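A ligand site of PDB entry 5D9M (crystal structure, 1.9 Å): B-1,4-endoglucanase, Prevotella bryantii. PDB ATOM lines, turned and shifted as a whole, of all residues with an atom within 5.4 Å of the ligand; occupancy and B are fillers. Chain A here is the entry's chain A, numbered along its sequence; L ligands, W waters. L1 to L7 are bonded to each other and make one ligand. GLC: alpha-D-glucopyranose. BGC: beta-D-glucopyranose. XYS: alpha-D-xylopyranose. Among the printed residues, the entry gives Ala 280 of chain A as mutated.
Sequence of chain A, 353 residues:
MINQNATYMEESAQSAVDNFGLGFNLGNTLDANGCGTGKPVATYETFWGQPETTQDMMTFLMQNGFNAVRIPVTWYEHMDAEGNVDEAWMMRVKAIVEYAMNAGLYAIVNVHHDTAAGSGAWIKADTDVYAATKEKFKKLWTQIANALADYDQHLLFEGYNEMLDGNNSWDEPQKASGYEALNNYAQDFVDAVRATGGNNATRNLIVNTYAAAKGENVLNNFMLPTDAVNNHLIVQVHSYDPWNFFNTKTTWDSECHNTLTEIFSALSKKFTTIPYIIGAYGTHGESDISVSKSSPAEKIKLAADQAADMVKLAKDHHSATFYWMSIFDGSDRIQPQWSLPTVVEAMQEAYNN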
ATOM      1  N   ASN A  28      -6.662  30.719  21.508  1.00  0.00           N
ATOM      2  CA  ASN A  28      -6.707  29.968  22.770  1.00  0.00           C
ATOM      3  C   ASN A  28      -5.982  30.734  23.866  1.00  0.00           C
ATOM      4  O   ASN A  28      -5.382  30.145  24.767  1.00  0.00           O
ATOM      5  CB  ASN A  28      -6.111  28.567  22.609  1.00  0.00           C
ATOM      6  CG  ASN A  28      -7.058  27.600  21.914  1.00  0.00           C
ATOM      7  OD1 ASN A  28      -8.126  27.976  21.428  1.00  0.00           O
ATOM      8  ND2 ASN A  28      -6.654  26.326  21.863  1.00  0.00           N
ATOM      9  N   ASP A  31      -9.082  34.364  24.356  1.00  0.00           N
ATOM     10  CA  ASP A  31     -10.360  33.748  24.002  1.00  0.00           C
ATOM     11  C   ASP A  31     -10.655  32.518  24.864  1.00  0.00           C
ATOM     12  O   ASP A  31     -11.785  32.025  24.883  1.00  0.00           O
ATOM     13  CB  ASP A  31     -10.396  33.370  22.516  1.00  0.00           C
ATOM     14  CG  ASP A  31      -9.117  32.732  22.024  1.00  0.00           C
ATOM     15  OD1 ASP A  31      -8.018  33.179  22.438  1.00  0.00           O
ATOM     16  OD2 ASP A  31      -9.192  31.784  21.197  1.00  0.00           O
ATOM     17  N   ASN A  33     -11.699  30.268  27.900  1.00  0.00           N
ATOM     18  CA  ASN A  33     -12.789  30.489  28.847  1.00  0.00           C
ATOM     19  C   ASN A  33     -13.275  29.181  29.459  1.00  0.00           C
ATOM     20  O   ASN A  33     -12.957  28.100  28.965  1.00  0.00           O
ATOM     21  CB  ASN A  33     -13.958  31.186  28.138  1.00  0.00           C
ATOM     22  CG  ASN A  33     -14.657  30.278  27.121  1.00  0.00           C
ATOM     23  OD1 ASN A  33     -15.683  29.657  27.433  1.00  0.00           O
ATOM     24  ND2 ASN A  33     -14.103  30.202  25.918  1.00  0.00           N
ATOM     25  N   GLY A  34     -14.051  29.288  30.539  1.00  0.00           N
ATOM     26  CA  GLY A  34     -14.652  28.120  31.158  1.00  0.00           C
ATOM     27  C   GLY A  34     -14.164  27.834  32.572  1.00  0.00           C
ATOM     28  O   GLY A  34     -14.630  26.886  33.202  1.00  0.00           O
ATOM     29  N   CYS A  35     -13.228  28.636  33.057  1.00  0.00           N
ATOM     30  CA  CYS A  35     -12.698  28.434  34.403  1.00  0.00           C
ATOM     31  C   CYS A  35     -13.542  29.150  35.463  1.00  0.00           C
ATOM     32  O   CYS A  35     -13.306  28.995  36.658  1.00  0.00           O
ATOM     33  CB  CYS A  35     -11.244  28.903  34.487  1.00  0.00           C
ATOM     34  SG  CYS A  35     -10.953  30.576  33.867  1.00  0.00           S
ATOM     35  N   PHE A  47      -5.480  29.335  30.575  1.00  0.00           N
ATOM     36  CA  PHE A  47      -6.404  28.239  30.882  1.00  0.00           C
ATOM     37  C   PHE A  47      -6.393  27.150  29.822  1.00  0.00           C
ATOM     38  O   PHE A  47      -6.655  25.984  30.127  1.00  0.00           O
ATOM     39  CB  PHE A  47      -7.832  28.785  31.059  1.00  0.00           C
ATOM     40  CG  PHE A  47      -8.809  27.769  31.581  1.00  0.00           C
ATOM     41  CD1 PHE A  47      -8.533  27.053  32.742  1.00  0.00           C
ATOM     42  CD2 PHE A  47     -10.008  27.536  30.931  1.00  0.00           C
ATOM     43  CE1 PHE A  47      -9.432  26.121  33.235  1.00  0.00           C
ATOM     44  CE2 PHE A  47     -10.916  26.612  31.418  1.00  0.00           C
ATOM     45  CZ  PHE A  47     -10.618  25.897  32.576  1.00  0.00           C
ATOM     46  N   TRP A  48      -6.083  27.504  28.579  1.00  0.00           N
ATOM     47  CA  TRP A  48      -6.085  26.532  27.482  1.00  0.00           C
ATOM     48  C   TRP A  48      -4.682  26.174  26.984  1.00  0.00           C
ATOM     49  O   TRP A  48      -4.514  25.804  25.824  1.00  0.00           O
ATOM     50  CB  TRP A  48      -6.930  27.056  26.321  1.00  0.00           C
ATOM     51  CG  TRP A  48      -8.403  26.975  26.588  1.00  0.00           C
ATOM     52  CD1 TRP A  48      -9.002  26.527  27.729  1.00  0.00           C
ATOM     53  CD2 TRP A  48      -9.459  27.361  25.701  1.00  0.00           C
ATOM     54  NE1 TRP A  48     -10.359  26.608  27.613  1.00  0.00           N
ATOM     55  CE2 TRP A  48     -10.669  27.113  26.379  1.00  0.00           C
ATOM     56  CE3 TRP A  48      -9.509  27.887  24.411  1.00  0.00           C
ATOM     57  CZ2 TRP A  48     -11.917  27.373  25.801  1.00  0.00           C
ATOM     58  CZ3 TRP A  48     -10.742  28.147  23.842  1.00  0.00           C
ATOM     59  CH2 TRP A  48     -11.928  27.892  24.536  1.00  0.00           C
ATOM     60  N   GLY A  49      -3.683  26.307  27.845  1.00  0.00           N
ATOM     61  CA  GLY A  49      -2.352  25.816  27.540  1.00  0.00           C
ATOM     62  C   GLY A  49      -1.377  26.763  26.869  1.00  0.00           C
ATOM     63  O   GLY A  49      -0.263  26.358  26.518  1.00  0.00           O
ATOM     64  N   HIS A 112     -15.184  36.933  20.870  1.00  0.00           N
ATOM     65  CA  HIS A 112     -14.953  35.594  20.321  1.00  0.00           C
ATOM     66  C   HIS A 112     -15.937  34.527  20.790  1.00  0.00           C
ATOM     67  O   HIS A 112     -17.005  34.377  20.203  1.00  0.00           O
ATOM     68  CB  HIS A 112     -13.512  35.154  20.625  1.00  0.00           C
ATOM     69  CG  HIS A 112     -12.966  34.149  19.654  1.00  0.00           C
ATOM     70  ND1 HIS A 112     -12.541  34.489  18.391  1.00  0.00           N
ATOM     71  CD2 HIS A 112     -12.800  32.807  19.757  1.00  0.00           C
ATOM     72  CE1 HIS A 112     -12.128  33.408  17.765  1.00  0.00           C
ATOM     73  NE2 HIS A 112     -12.275  32.376  18.572  1.00  0.00           N
ATOM     74  N   HIS A 113     -15.604  33.767  21.838  1.00  0.00           N
ATOM     75  CA  HIS A 113     -16.459  32.636  22.231  1.00  0.00           C
ATOM     76  C   HIS A 113     -17.705  33.065  22.991  1.00  0.00           C
ATOM     77  O   HIS A 113     -18.421  32.240  23.562  1.00  0.00           O
ATOM     78  CB  HIS A 113     -15.668  31.622  23.039  1.00  0.00           C
ATOM     79  CG  HIS A 113     -14.657  30.867  22.226  1.00  0.00           C
ATOM     80  ND1 HIS A 113     -14.930  30.443  20.934  1.00  0.00           N
ATOM     81  CD2 HIS A 113     -13.395  30.485  22.499  1.00  0.00           C
ATOM     82  CE1 HIS A 113     -13.861  29.815  20.462  1.00  0.00           C
ATOM     83  NE2 HIS A 113     -12.922  29.828  21.389  1.00  0.00           N
ATOM     84  N   THR A 115     -19.731  34.096  21.054  1.00  0.00           N
ATOM     85  CA  THR A 115     -20.495  33.514  19.952  1.00  0.00           C
ATOM     86  C   THR A 115     -20.226  32.018  19.824  1.00  0.00           C
ATOM     87  O   THR A 115     -19.230  31.514  20.352  1.00  0.00           O
ATOM     88  CB  THR A 115     -20.170  34.167  18.593  1.00  0.00           C
ATOM     89  OG1 THR A 115     -18.805  33.887  18.253  1.00  0.00           O
ATOM     90  CG2 THR A 115     -20.375  35.668  18.628  1.00  0.00           C
ATOM     91  N   ALA A 116     -21.139  31.341  19.117  1.00  0.00           N
ATOM     92  CA  ALA A 116     -20.999  29.986  18.562  1.00  0.00           C
ATOM     93  C   ALA A 116     -21.516  28.883  19.482  1.00  0.00           C
ATOM     94  O   ALA A 116     -22.525  29.055  20.181  1.00  0.00           O
ATOM     95  CB  ALA A 116     -19.534  29.691  18.159  1.00  0.00           C
ATOM     96  N   ALA A 117     -20.841  27.738  19.463  1.00  0.00           N
ATOM     97  CA  ALA A 117     -21.461  26.487  19.897  1.00  0.00           C
ATOM     98  C   ALA A 117     -21.058  26.063  21.296  1.00  0.00           C
ATOM     99  O   ALA A 117     -21.529  25.030  21.792  1.00  0.00           O
ATOM    100  CB  ALA A 117     -21.137  25.385  18.891  1.00  0.00           C
ATOM    101  N   GLY A 118     -20.197  26.845  21.934  1.00  0.00           N
ATOM    102  CA  GLY A 118     -19.733  26.517  23.268  1.00  0.00           C
ATOM    103  C   GLY A 118     -20.632  27.017  24.375  1.00  0.00           C
ATOM    104  O   GLY A 118     -21.494  27.868  24.162  1.00  0.00           O
ATOM    105  N   ASN A 161     -17.276  36.914  16.380  1.00  0.00           N
ATOM    106  CA  ASN A 161     -16.496  35.867  15.723  1.00  0.00           C
ATOM    107  C   ASN A 161     -17.324  34.974  14.783  1.00  0.00           C
ATOM    108  O   ASN A 161     -17.350  35.189  13.577  1.00  0.00           O
ATOM    109  CB  ASN A 161     -15.802  35.007  16.782  1.00  0.00           C
ATOM    110  CG  ASN A 161     -14.983  33.874  16.194  1.00  0.00           C
ATOM    111  OD1 ASN A 161     -14.247  34.057  15.230  1.00  0.00           O
ATOM    112  ND2 ASN A 161     -15.110  32.698  16.785  1.00  0.00           N
ATOM    113  N   GLU A 162     -17.966  33.969  15.356  1.00  0.00           N
ATOM    114  CA  GLU A 162     -18.739  33.015  14.569  1.00  0.00           C
ATOM    115  C   GLU A 162     -20.143  32.877  15.131  1.00  0.00           C
ATOM    116  O   GLU A 162     -20.453  31.922  15.859  1.00  0.00           O
ATOM    117  CB  GLU A 162     -18.017  31.661  14.510  1.00  0.00           C
ATOM    118  CG  GLU A 162     -16.688  31.754  13.786  1.00  0.00           C
ATOM    119  CD  GLU A 162     -15.847  30.496  13.840  1.00  0.00           C
ATOM    120  OE1 GLU A 162     -16.157  29.592  14.633  1.00  0.00           O
ATOM    121  OE2 GLU A 162     -14.842  30.437  13.102  1.00  0.00           O
ATOM    122  N   TRP A 170     -23.759  25.294  12.088  1.00  0.00           N
ATOM    123  CA  TRP A 170     -22.593  25.715  11.336  1.00  0.00           C
ATOM    124  C   TRP A 170     -22.953  25.917   9.871  1.00  0.00           C
ATOM    125  O   TRP A 170     -23.978  25.419   9.404  1.00  0.00           O
ATOM    126  CB  TRP A 170     -21.455  24.702  11.468  1.00  0.00           C
ATOM    127  CG  TRP A 170     -20.905  24.631  12.855  1.00  0.00           C
ATOM    128  CD1 TRP A 170     -21.062  23.610  13.755  1.00  0.00           C
ATOM    129  CD2 TRP A 170     -20.115  25.631  13.518  1.00  0.00           C
ATOM    130  NE1 TRP A 170     -20.414  23.909  14.926  1.00  0.00           N
ATOM    131  CE2 TRP A 170     -19.824  25.139  14.815  1.00  0.00           C
ATOM    132  CE3 TRP A 170     -19.635  26.884  13.145  1.00  0.00           C
ATOM    133  CZ2 TRP A 170     -19.069  25.876  15.731  1.00  0.00           C
ATOM    134  CZ3 TRP A 170     -18.876  27.608  14.056  1.00  0.00           C
ATOM    135  CH2 TRP A 170     -18.610  27.100  15.338  1.00  0.00           C
ATOM    136  N   HIS A 238     -14.028  32.697   7.555  1.00  0.00           N
ATOM    137  CA  HIS A 238     -13.009  31.737   7.986  1.00  0.00           C
ATOM    138  C   HIS A 238     -12.966  30.588   7.006  1.00  0.00           C
ATOM    139  O   HIS A 238     -13.874  30.443   6.194  1.00  0.00           O
ATOM    140  CB  HIS A 238     -13.308  31.244   9.399  1.00  0.00           C
ATOM    141  CG  HIS A 238     -13.240  32.316  10.443  1.00  0.00           C
ATOM    142  ND1 HIS A 238     -13.733  32.161  11.715  1.00  0.00           N
ATOM    143  CD2 HIS A 238     -12.715  33.565  10.391  1.00  0.00           C
ATOM    144  CE1 HIS A 238     -13.529  33.272  12.409  1.00  0.00           C
ATOM    145  NE2 HIS A 238     -12.912  34.133  11.626  1.00  0.00           N
ATOM    146  N   TYR A 240     -11.471  26.325   6.676  1.00  0.00           N
ATOM    147  CA  TYR A 240     -10.682  25.141   6.921  1.00  0.00           C
ATOM    148  C   TYR A 240     -10.991  24.163   5.783  1.00  0.00           C
ATOM    149  O   TYR A 240     -11.063  22.952   5.991  1.00  0.00           O
ATOM    150  CB  TYR A 240     -10.989  24.554   8.306  1.00  0.00           C
ATOM    151  CG  TYR A 240     -10.627  25.528   9.403  1.00  0.00           C
ATOM    152  CD1 TYR A 240     -11.536  26.489   9.832  1.00  0.00           C
ATOM    153  CD2 TYR A 240      -9.364  25.517   9.975  1.00  0.00           C
ATOM    154  CE1 TYR A 240     -11.202  27.406  10.822  1.00  0.00           C
ATOM    155  CE2 TYR A 240      -9.017  26.413  10.965  1.00  0.00           C
ATOM    156  CZ  TYR A 240      -9.935  27.358  11.388  1.00  0.00           C
ATOM    157  OH  TYR A 240      -9.596  28.259  12.381  1.00  0.00           O
ATOM    158  N   ALA A 280      -9.302  33.464   9.830  1.00  0.00           N
ATOM    159  CA  ALA A 280      -8.798  32.272  10.489  1.00  0.00           C
ATOM    160  C   ALA A 280      -8.792  31.124   9.503  1.00  0.00           C
ATOM    161  O   ALA A 280      -9.782  30.885   8.825  1.00  0.00           O
ATOM    162  CB  ALA A 280      -9.655  31.926  11.716  1.00  0.00           C
ATOM    163  N   HIS A 284      -7.264  22.401  10.905  1.00  0.00           N
ATOM    164  CA  HIS A 284      -8.192  21.870  11.910  1.00  0.00           C
ATOM    165  C   HIS A 284      -9.437  21.218  11.286  1.00  0.00           C
ATOM    166  O   HIS A 284     -10.204  21.875  10.587  1.00  0.00           O
ATOM    167  CB  HIS A 284      -8.622  22.980  12.867  1.00  0.00           C
ATOM    168  CG  HIS A 284      -7.458  23.634  13.556  1.00  0.00           C
ATOM    169  ND1 HIS A 284      -6.535  24.407  12.883  1.00  0.00           N
ATOM    170  CD2 HIS A 284      -7.063  23.616  14.854  1.00  0.00           C
ATOM    171  CE1 HIS A 284      -5.624  24.842  13.730  1.00  0.00           C
ATOM    172  NE2 HIS A 284      -5.922  24.373  14.934  1.00  0.00           N
ATOM    173  N   ASP A 288     -11.361  18.374  15.741  1.00  0.00           N
ATOM    174  CA  ASP A 288     -10.329  19.401  15.795  1.00  0.00           C
ATOM    175  C   ASP A 288      -8.911  18.838  15.755  1.00  0.00           C
ATOM    176  O   ASP A 288      -7.996  19.410  16.342  1.00  0.00           O
ATOM    177  CB  ASP A 288     -10.494  20.288  17.041  1.00  0.00           C
ATOM    178  CG  ASP A 288     -10.071  21.732  16.778  1.00  0.00           C
ATOM    179  OD1 ASP A 288     -10.617  22.340  15.835  1.00  0.00           O
ATOM    180  OD2 ASP A 288      -9.192  22.251  17.511  1.00  0.00           O
ATOM    181  N   TRP A 324      -4.560  30.334  11.926  1.00  0.00           N
ATOM    182  CA  TRP A 324      -5.075  29.926  13.226  1.00  0.00           C
ATOM    183  C   TRP A 324      -4.066  29.048  13.999  1.00  0.00           C
ATOM    184  O   TRP A 324      -4.029  27.818  13.826  1.00  0.00           O
ATOM    185  CB  TRP A 324      -6.409  29.174  13.117  1.00  0.00           C
ATOM    186  CG  TRP A 324      -6.964  28.854  14.481  1.00  0.00           C
ATOM    187  CD1 TRP A 324      -6.994  27.624  15.091  1.00  0.00           C
ATOM    188  CD2 TRP A 324      -7.501  29.776  15.427  1.00  0.00           C
ATOM    189  NE1 TRP A 324      -7.544  27.738  16.354  1.00  0.00           N
ATOM    190  CE2 TRP A 324      -7.862  29.045  16.583  1.00  0.00           C
ATOM    191  CE3 TRP A 324      -7.737  31.158  15.404  1.00  0.00           C
ATOM    192  CZ2 TRP A 324      -8.425  29.654  17.706  1.00  0.00           C
ATOM    193  CZ3 TRP A 324      -8.296  31.754  16.521  1.00  0.00           C
ATOM    194  CH2 TRP A 324      -8.637  31.006  17.657  1.00  0.00           C
ATOM    195  N   MET A 325      -3.244  29.712  14.800  1.00  0.00           N
ATOM    196  CA  MET A 325      -2.507  29.131  15.928  1.00  0.00           C
ATOM    197  C   MET A 325      -1.256  28.285  15.625  1.00  0.00           C
ATOM    198  O   MET A 325      -0.205  28.517  16.216  1.00  0.00           O
ATOM    199  CB  MET A 325      -3.452  28.283  16.790  1.00  0.00           C
ATOM    200  CG  MET A 325      -4.442  29.067  17.624  1.00  0.00           C
ATOM    201  SD  MET A 325      -5.293  28.047  18.850  1.00  0.00           S
ATOM    202  CE  MET A 325      -3.916  27.594  19.898  1.00  0.00           C
HETATM  203  C1  GLC L   1     -12.460  28.799  14.413  1.00  0.00           C
HETATM  204  C2  GLC L   1     -12.812  29.189  15.833  1.00  0.00           C
HETATM  205  C3  GLC L   1     -11.638  28.906  16.748  1.00  0.00           C
HETATM  206  C4  GLC L   1     -11.290  27.419  16.669  1.00  0.00           C
HETATM  207  C5  GLC L   1     -10.882  27.162  15.222  1.00  0.00           C
HETATM  208  C6  GLC L   1     -10.410  25.728  15.019  1.00  0.00           C
HETATM  209  O1  GLC L   1     -11.459  29.680  13.886  1.00  0.00           O
HETATM  210  O2  GLC L   1     -13.135  30.593  15.863  1.00  0.00           O
HETATM  211  O3  GLC L   1     -11.973  29.290  18.087  1.00  0.00           O
HETATM  212  O4  GLC L   1     -10.187  27.123  17.533  1.00  0.00           O
HETATM  213  O5  GLC L   1     -12.021  27.426  14.371  1.00  0.00           O
HETATM  214  O6  GLC L   1     -11.479  24.826  15.371  1.00  0.00           O
HETATM  215  C2  BGC L   2      -9.151  25.598  19.035  1.00  0.00           C
HETATM  216  C3  BGC L   2      -9.383  24.478  20.033  1.00  0.00           C
HETATM  217  C4  BGC L   2     -10.358  24.962  21.111  1.00  0.00           C
HETATM  218  C5  BGC L   2     -11.640  25.390  20.389  1.00  0.00           C
HETATM  219  C6  BGC L   2     -12.719  25.823  21.371  1.00  0.00           C
HETATM  220  C1  BGC L   2     -10.470  26.050  18.449  1.00  0.00           C
HETATM  221  O2  BGC L   2      -8.307  25.111  17.984  1.00  0.00           O
HETATM  222  O3  BGC L   2      -8.136  24.071  20.615  1.00  0.00           O
HETATM  223  O4  BGC L   2     -10.666  23.875  21.969  1.00  0.00           O
HETATM  224  O5  BGC L   2     -11.355  26.479  19.492  1.00  0.00           O
HETATM  225  O6  BGC L   2     -13.989  25.657  20.725  1.00  0.00           O
HETATM  226  C2  BGC L   3     -10.979  23.304  24.267  1.00  0.00           C
HETATM  227  C3  BGC L   3     -10.407  23.462  25.661  1.00  0.00           C
HETATM  228  C4  BGC L   3      -8.931  23.027  25.679  1.00  0.00           C
HETATM  229  C5  BGC L   3      -8.207  23.827  24.605  1.00  0.00           C
HETATM  230  C6  BGC L   3      -6.731  23.419  24.547  1.00  0.00           C
HETATM  231  C1  BGC L   3     -10.132  24.085  23.280  1.00  0.00           C
HETATM  232  O2  BGC L   3     -12.320  23.804  24.249  1.00  0.00           O
HETATM  233  O3  BGC L   3     -11.225  22.679  26.568  1.00  0.00           O
HETATM  234  O4  BGC L   3      -8.279  23.364  26.909  1.00  0.00           O
HETATM  235  O5  BGC L   3      -8.804  23.603  23.339  1.00  0.00           O
HETATM  236  O6  BGC L   3      -6.640  22.131  23.917  1.00  0.00           O
HETATM  237  C1  XYS L   4     -15.045  25.612  21.710  1.00  0.00           C
HETATM  238  C2  XYS L   4     -16.109  24.592  21.269  1.00  0.00           C
HETATM  239  C3  XYS L   4     -16.742  25.045  19.976  1.00  0.00           C
HETATM  240  C4  XYS L   4     -17.358  26.415  20.192  1.00  0.00           C
HETATM  241  C5  XYS L   4     -16.249  27.383  20.638  1.00  0.00           C
HETATM  242  O2  XYS L   4     -15.503  23.308  21.069  1.00  0.00           O
HETATM  243  O3  XYS L   4     -17.778  24.108  19.600  1.00  0.00           O
HETATM  244  O4  XYS L   4     -17.956  26.874  18.963  1.00  0.00           O
HETATM  245  O5  XYS L   4     -15.655  26.912  21.873  1.00  0.00           O
HETATM  246  C2  BGC L   5      -7.297  22.523  28.924  1.00  0.00           C
HETATM  247  C3  BGC L   5      -7.559  21.758  30.217  1.00  0.00           C
HETATM  248  C4  BGC L   5      -8.801  22.323  30.859  1.00  0.00           C
HETATM  249  C5  BGC L   5      -9.945  22.155  29.892  1.00  0.00           C
HETATM  250  C6  BGC L   5     -11.239  22.719  30.485  1.00  0.00           C
HETATM  251  C1  BGC L   5      -8.523  22.484  28.010  1.00  0.00           C
HETATM  252  O2  BGC L   5      -6.172  21.933  28.242  1.00  0.00           O
HETATM  253  O3  BGC L   5      -6.443  21.895  31.110  1.00  0.00           O
HETATM  254  O4  BGC L   5      -9.073  21.613  32.078  1.00  0.00           O
HETATM  255  O5  BGC L   5      -9.692  22.902  28.701  1.00  0.00           O
HETATM  256  O6  BGC L   5     -12.266  22.506  29.517  1.00  0.00           O
HETATM  257  C1  XYS L   6      -5.301  21.937  23.408  1.00  0.00           C
HETATM  258  C2  XYS L   6      -5.270  20.654  22.591  1.00  0.00           C
HETATM  259  C3  XYS L   6      -5.638  19.495  23.481  1.00  0.00           C
HETATM  260  C4  XYS L   6      -4.643  19.419  24.604  1.00  0.00           C
HETATM  261  C5  XYS L   6      -4.662  20.737  25.369  1.00  0.00           C
HETATM  262  O2  XYS L   6      -6.224  20.744  21.534  1.00  0.00           O
HETATM  263  O3  XYS L   6      -5.610  18.271  22.744  1.00  0.00           O
HETATM  264  O4  XYS L   6      -5.012  18.337  25.483  1.00  0.00           O
HETATM  265  O5  XYS L   6      -4.336  21.835  24.481  1.00  0.00           O
HETATM  266  C1  XYS L   7     -13.532  22.977  30.013  1.00  0.00           C
HETATM  267  C2  XYS L   7     -14.621  22.219  29.281  1.00  0.00           C
HETATM  268  C3  XYS L   7     -14.501  22.515  27.797  1.00  0.00           C
HETATM  269  C4  XYS L   7     -14.581  24.020  27.567  1.00  0.00           C
HETATM  270  C5  XYS L   7     -13.515  24.729  28.411  1.00  0.00           C
HETATM  271  O2  XYS L   7     -14.452  20.814  29.488  1.00  0.00           O
HETATM  272  O3  XYS L   7     -15.559  21.855  27.081  1.00  0.00           O
HETATM  273  O4  XYS L   7     -14.354  24.302  26.183  1.00  0.00           O
HETATM  274  O5  XYS L   7     -13.697  24.390  29.809  1.00  0.00           O
HETATM  275  O   HOH W   1      -6.180  23.605  33.031  1.00  0.00           O
HETATM  276  O   HOH W   2     -10.354  29.369  20.345  1.00  0.00           O
HETATM  277  O   HOH W   3     -16.455  25.590  25.008  1.00  0.00           O
HETATM  278  O   HOH W   4     -11.320  32.269  14.860  1.00  0.00           O
HETATM  279  O   HOH W   5     -15.309  21.032  24.236  1.00  0.00           O
HETATM  280  O   HOH W   6     -17.986  23.064  27.998  1.00  0.00           O
HETATM  281  O   HOH W   7      -2.016  22.366  26.112  1.00  0.00           O
HETATM  282  O   HOH W   8     -19.531  22.946  21.226  1.00  0.00           O
HETATM  283  O   HOH W   9      -5.135  19.299  19.198  1.00  0.00           O
HETATM  284  O   HOH W  10      -4.056  23.083  27.844  1.00  0.00           O
HETATM  285  O   HOH W  11      -6.006  23.319  19.141  1.00  0.00           O
HETATM  286  O   HOH W  12     -15.747  28.248  24.260  1.00  0.00           O
HETATM  287  O   HOH W  13     -13.677  22.157  22.543  1.00  0.00           O
HETATM  288  O   HOH W  14     -16.225  28.991  17.435  1.00  0.00           O
HETATM  289  O   HOH W  15     -17.535  22.706  17.560  1.00  0.00           O
HETATM  290  O   HOH W  16      -2.940  18.130  27.073  1.00  0.00           O
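The side-chain sulfur of Met 325 lies within hydrogen-bond range of the indole nitrogen of Trp 324.
The backbone NH (N) of Asn 28 is in hydrogen-bond range of the side-chain carboxylate (OD2) of Asp 31.
The side-chain hydroxyl of Thr 115 is in hydrogen-bond range of the backbone carbonyl oxygen of His 112, 2.7 Å away.
The backbone carbonyl oxygen (O) of Glu 162 sits close to the backbone NH (N) of Ala 116, 3.4 Å away.
The side-chain carboxylate (OE2) of Glu 162 sits at hydrogen-bond distance from a ring nitrogen (ND1) of His 238 (2.5 Å).
OG1 of Thr 115 sits at hydrogen-bond distance from N of Glu 162, 3.0 Å away.
The indole nitrogen (NE1) of Trp 48 lies within hydrogen-bond range of the backbone carbonyl oxygen (O) of Asn 33 (3.3 Å).
The side-chain amide nitrogen (ND2) of Asn 33 sits at hydrogen-bond distance from the backbone carbonyl oxygen (O) of Asp 31 (3.1 Å).
O6 of GLC L1 lies within hydrogen-bond range of OD1 of Asp 288.
The side-chain hydroxyl (OH) of Tyr 240 lies within hydrogen-bond range of an oxygen (O1) of GLC L1.
An oxygen (O4) of GLC L1 sits at hydrogen-bond distance from the indole nitrogen (NE1) of Trp 324, 3.0 Å away.
The side-chain amide nitrogen (ND2) of Asn 28 lies within hydrogen-bond range of an oxygen (O3) of BGC L2 (3.0 Å).
The side-chain amide nitrogen (ND2) of Asn 161 lies within hydrogen-bond range of an oxygen (O2) of GLC L1 (3.0 Å).
An oxygen (O4) of XYS L4 lies within hydrogen-bond range of the backbone NH (N) of Ala 117, at 3.1 Å.
NE2 of His 113 lies close to O3 of GLC L1, at 3.5 Å.
A ring nitrogen (NE2) of His 112 is in hydrogen-bond range of an oxygen (O3) of GLC L1, 3.1 Å away.
The side-chain carboxylate (OE2) of Glu 162 sits close to an oxygen (O2) of GLC L1, 3.2 Å away.
Water W10 lies within hydrogen-bond range of O2 of BGC L5 (2.4 Å), N of Gly 49 (3.2 Å) and O of Trp 48 (3.4 Å).
Water W8 lies within hydrogen-bond range of an oxygen (O3) of XYS L4 and the backbone carbonyl oxygen of Ala 117.
Water W4 lies within hydrogen-bond range of O2 of GLC L1 (2.7 Å) and OD1 of Asn 161 (3.4 Å).
Water W12 bridges an oxygen (O5) of XYS L4 (2.7 Å) and the side-chain amide nitrogen (ND2) of Asn 33 (3.0 Å).
Water W2 lies within hydrogen-bond range of O3 of GLC L1 (2.8 Å), NE2 of His 113 (2.8 Å), OD2 of Asp 31 (2.8 Å) and OD1 of Asn 28 (2.8 Å).
Water W14 bridges the side-chain carboxylate of Glu 162 (2.9 Å) and an oxygen (O4) of XYS L4 (3.1 Å).
Merely in contact with the ligand: Ala 116 (3.3 Å), Trp 48 (3.3 Å), Gly 118 (3.4 Å), Asn 33 (3.5 Å), Trp 170 (3.6 Å), Ala 280 (3.6 Å), His 284 (3.7 Å) and Phe 47 (3.7 Å).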
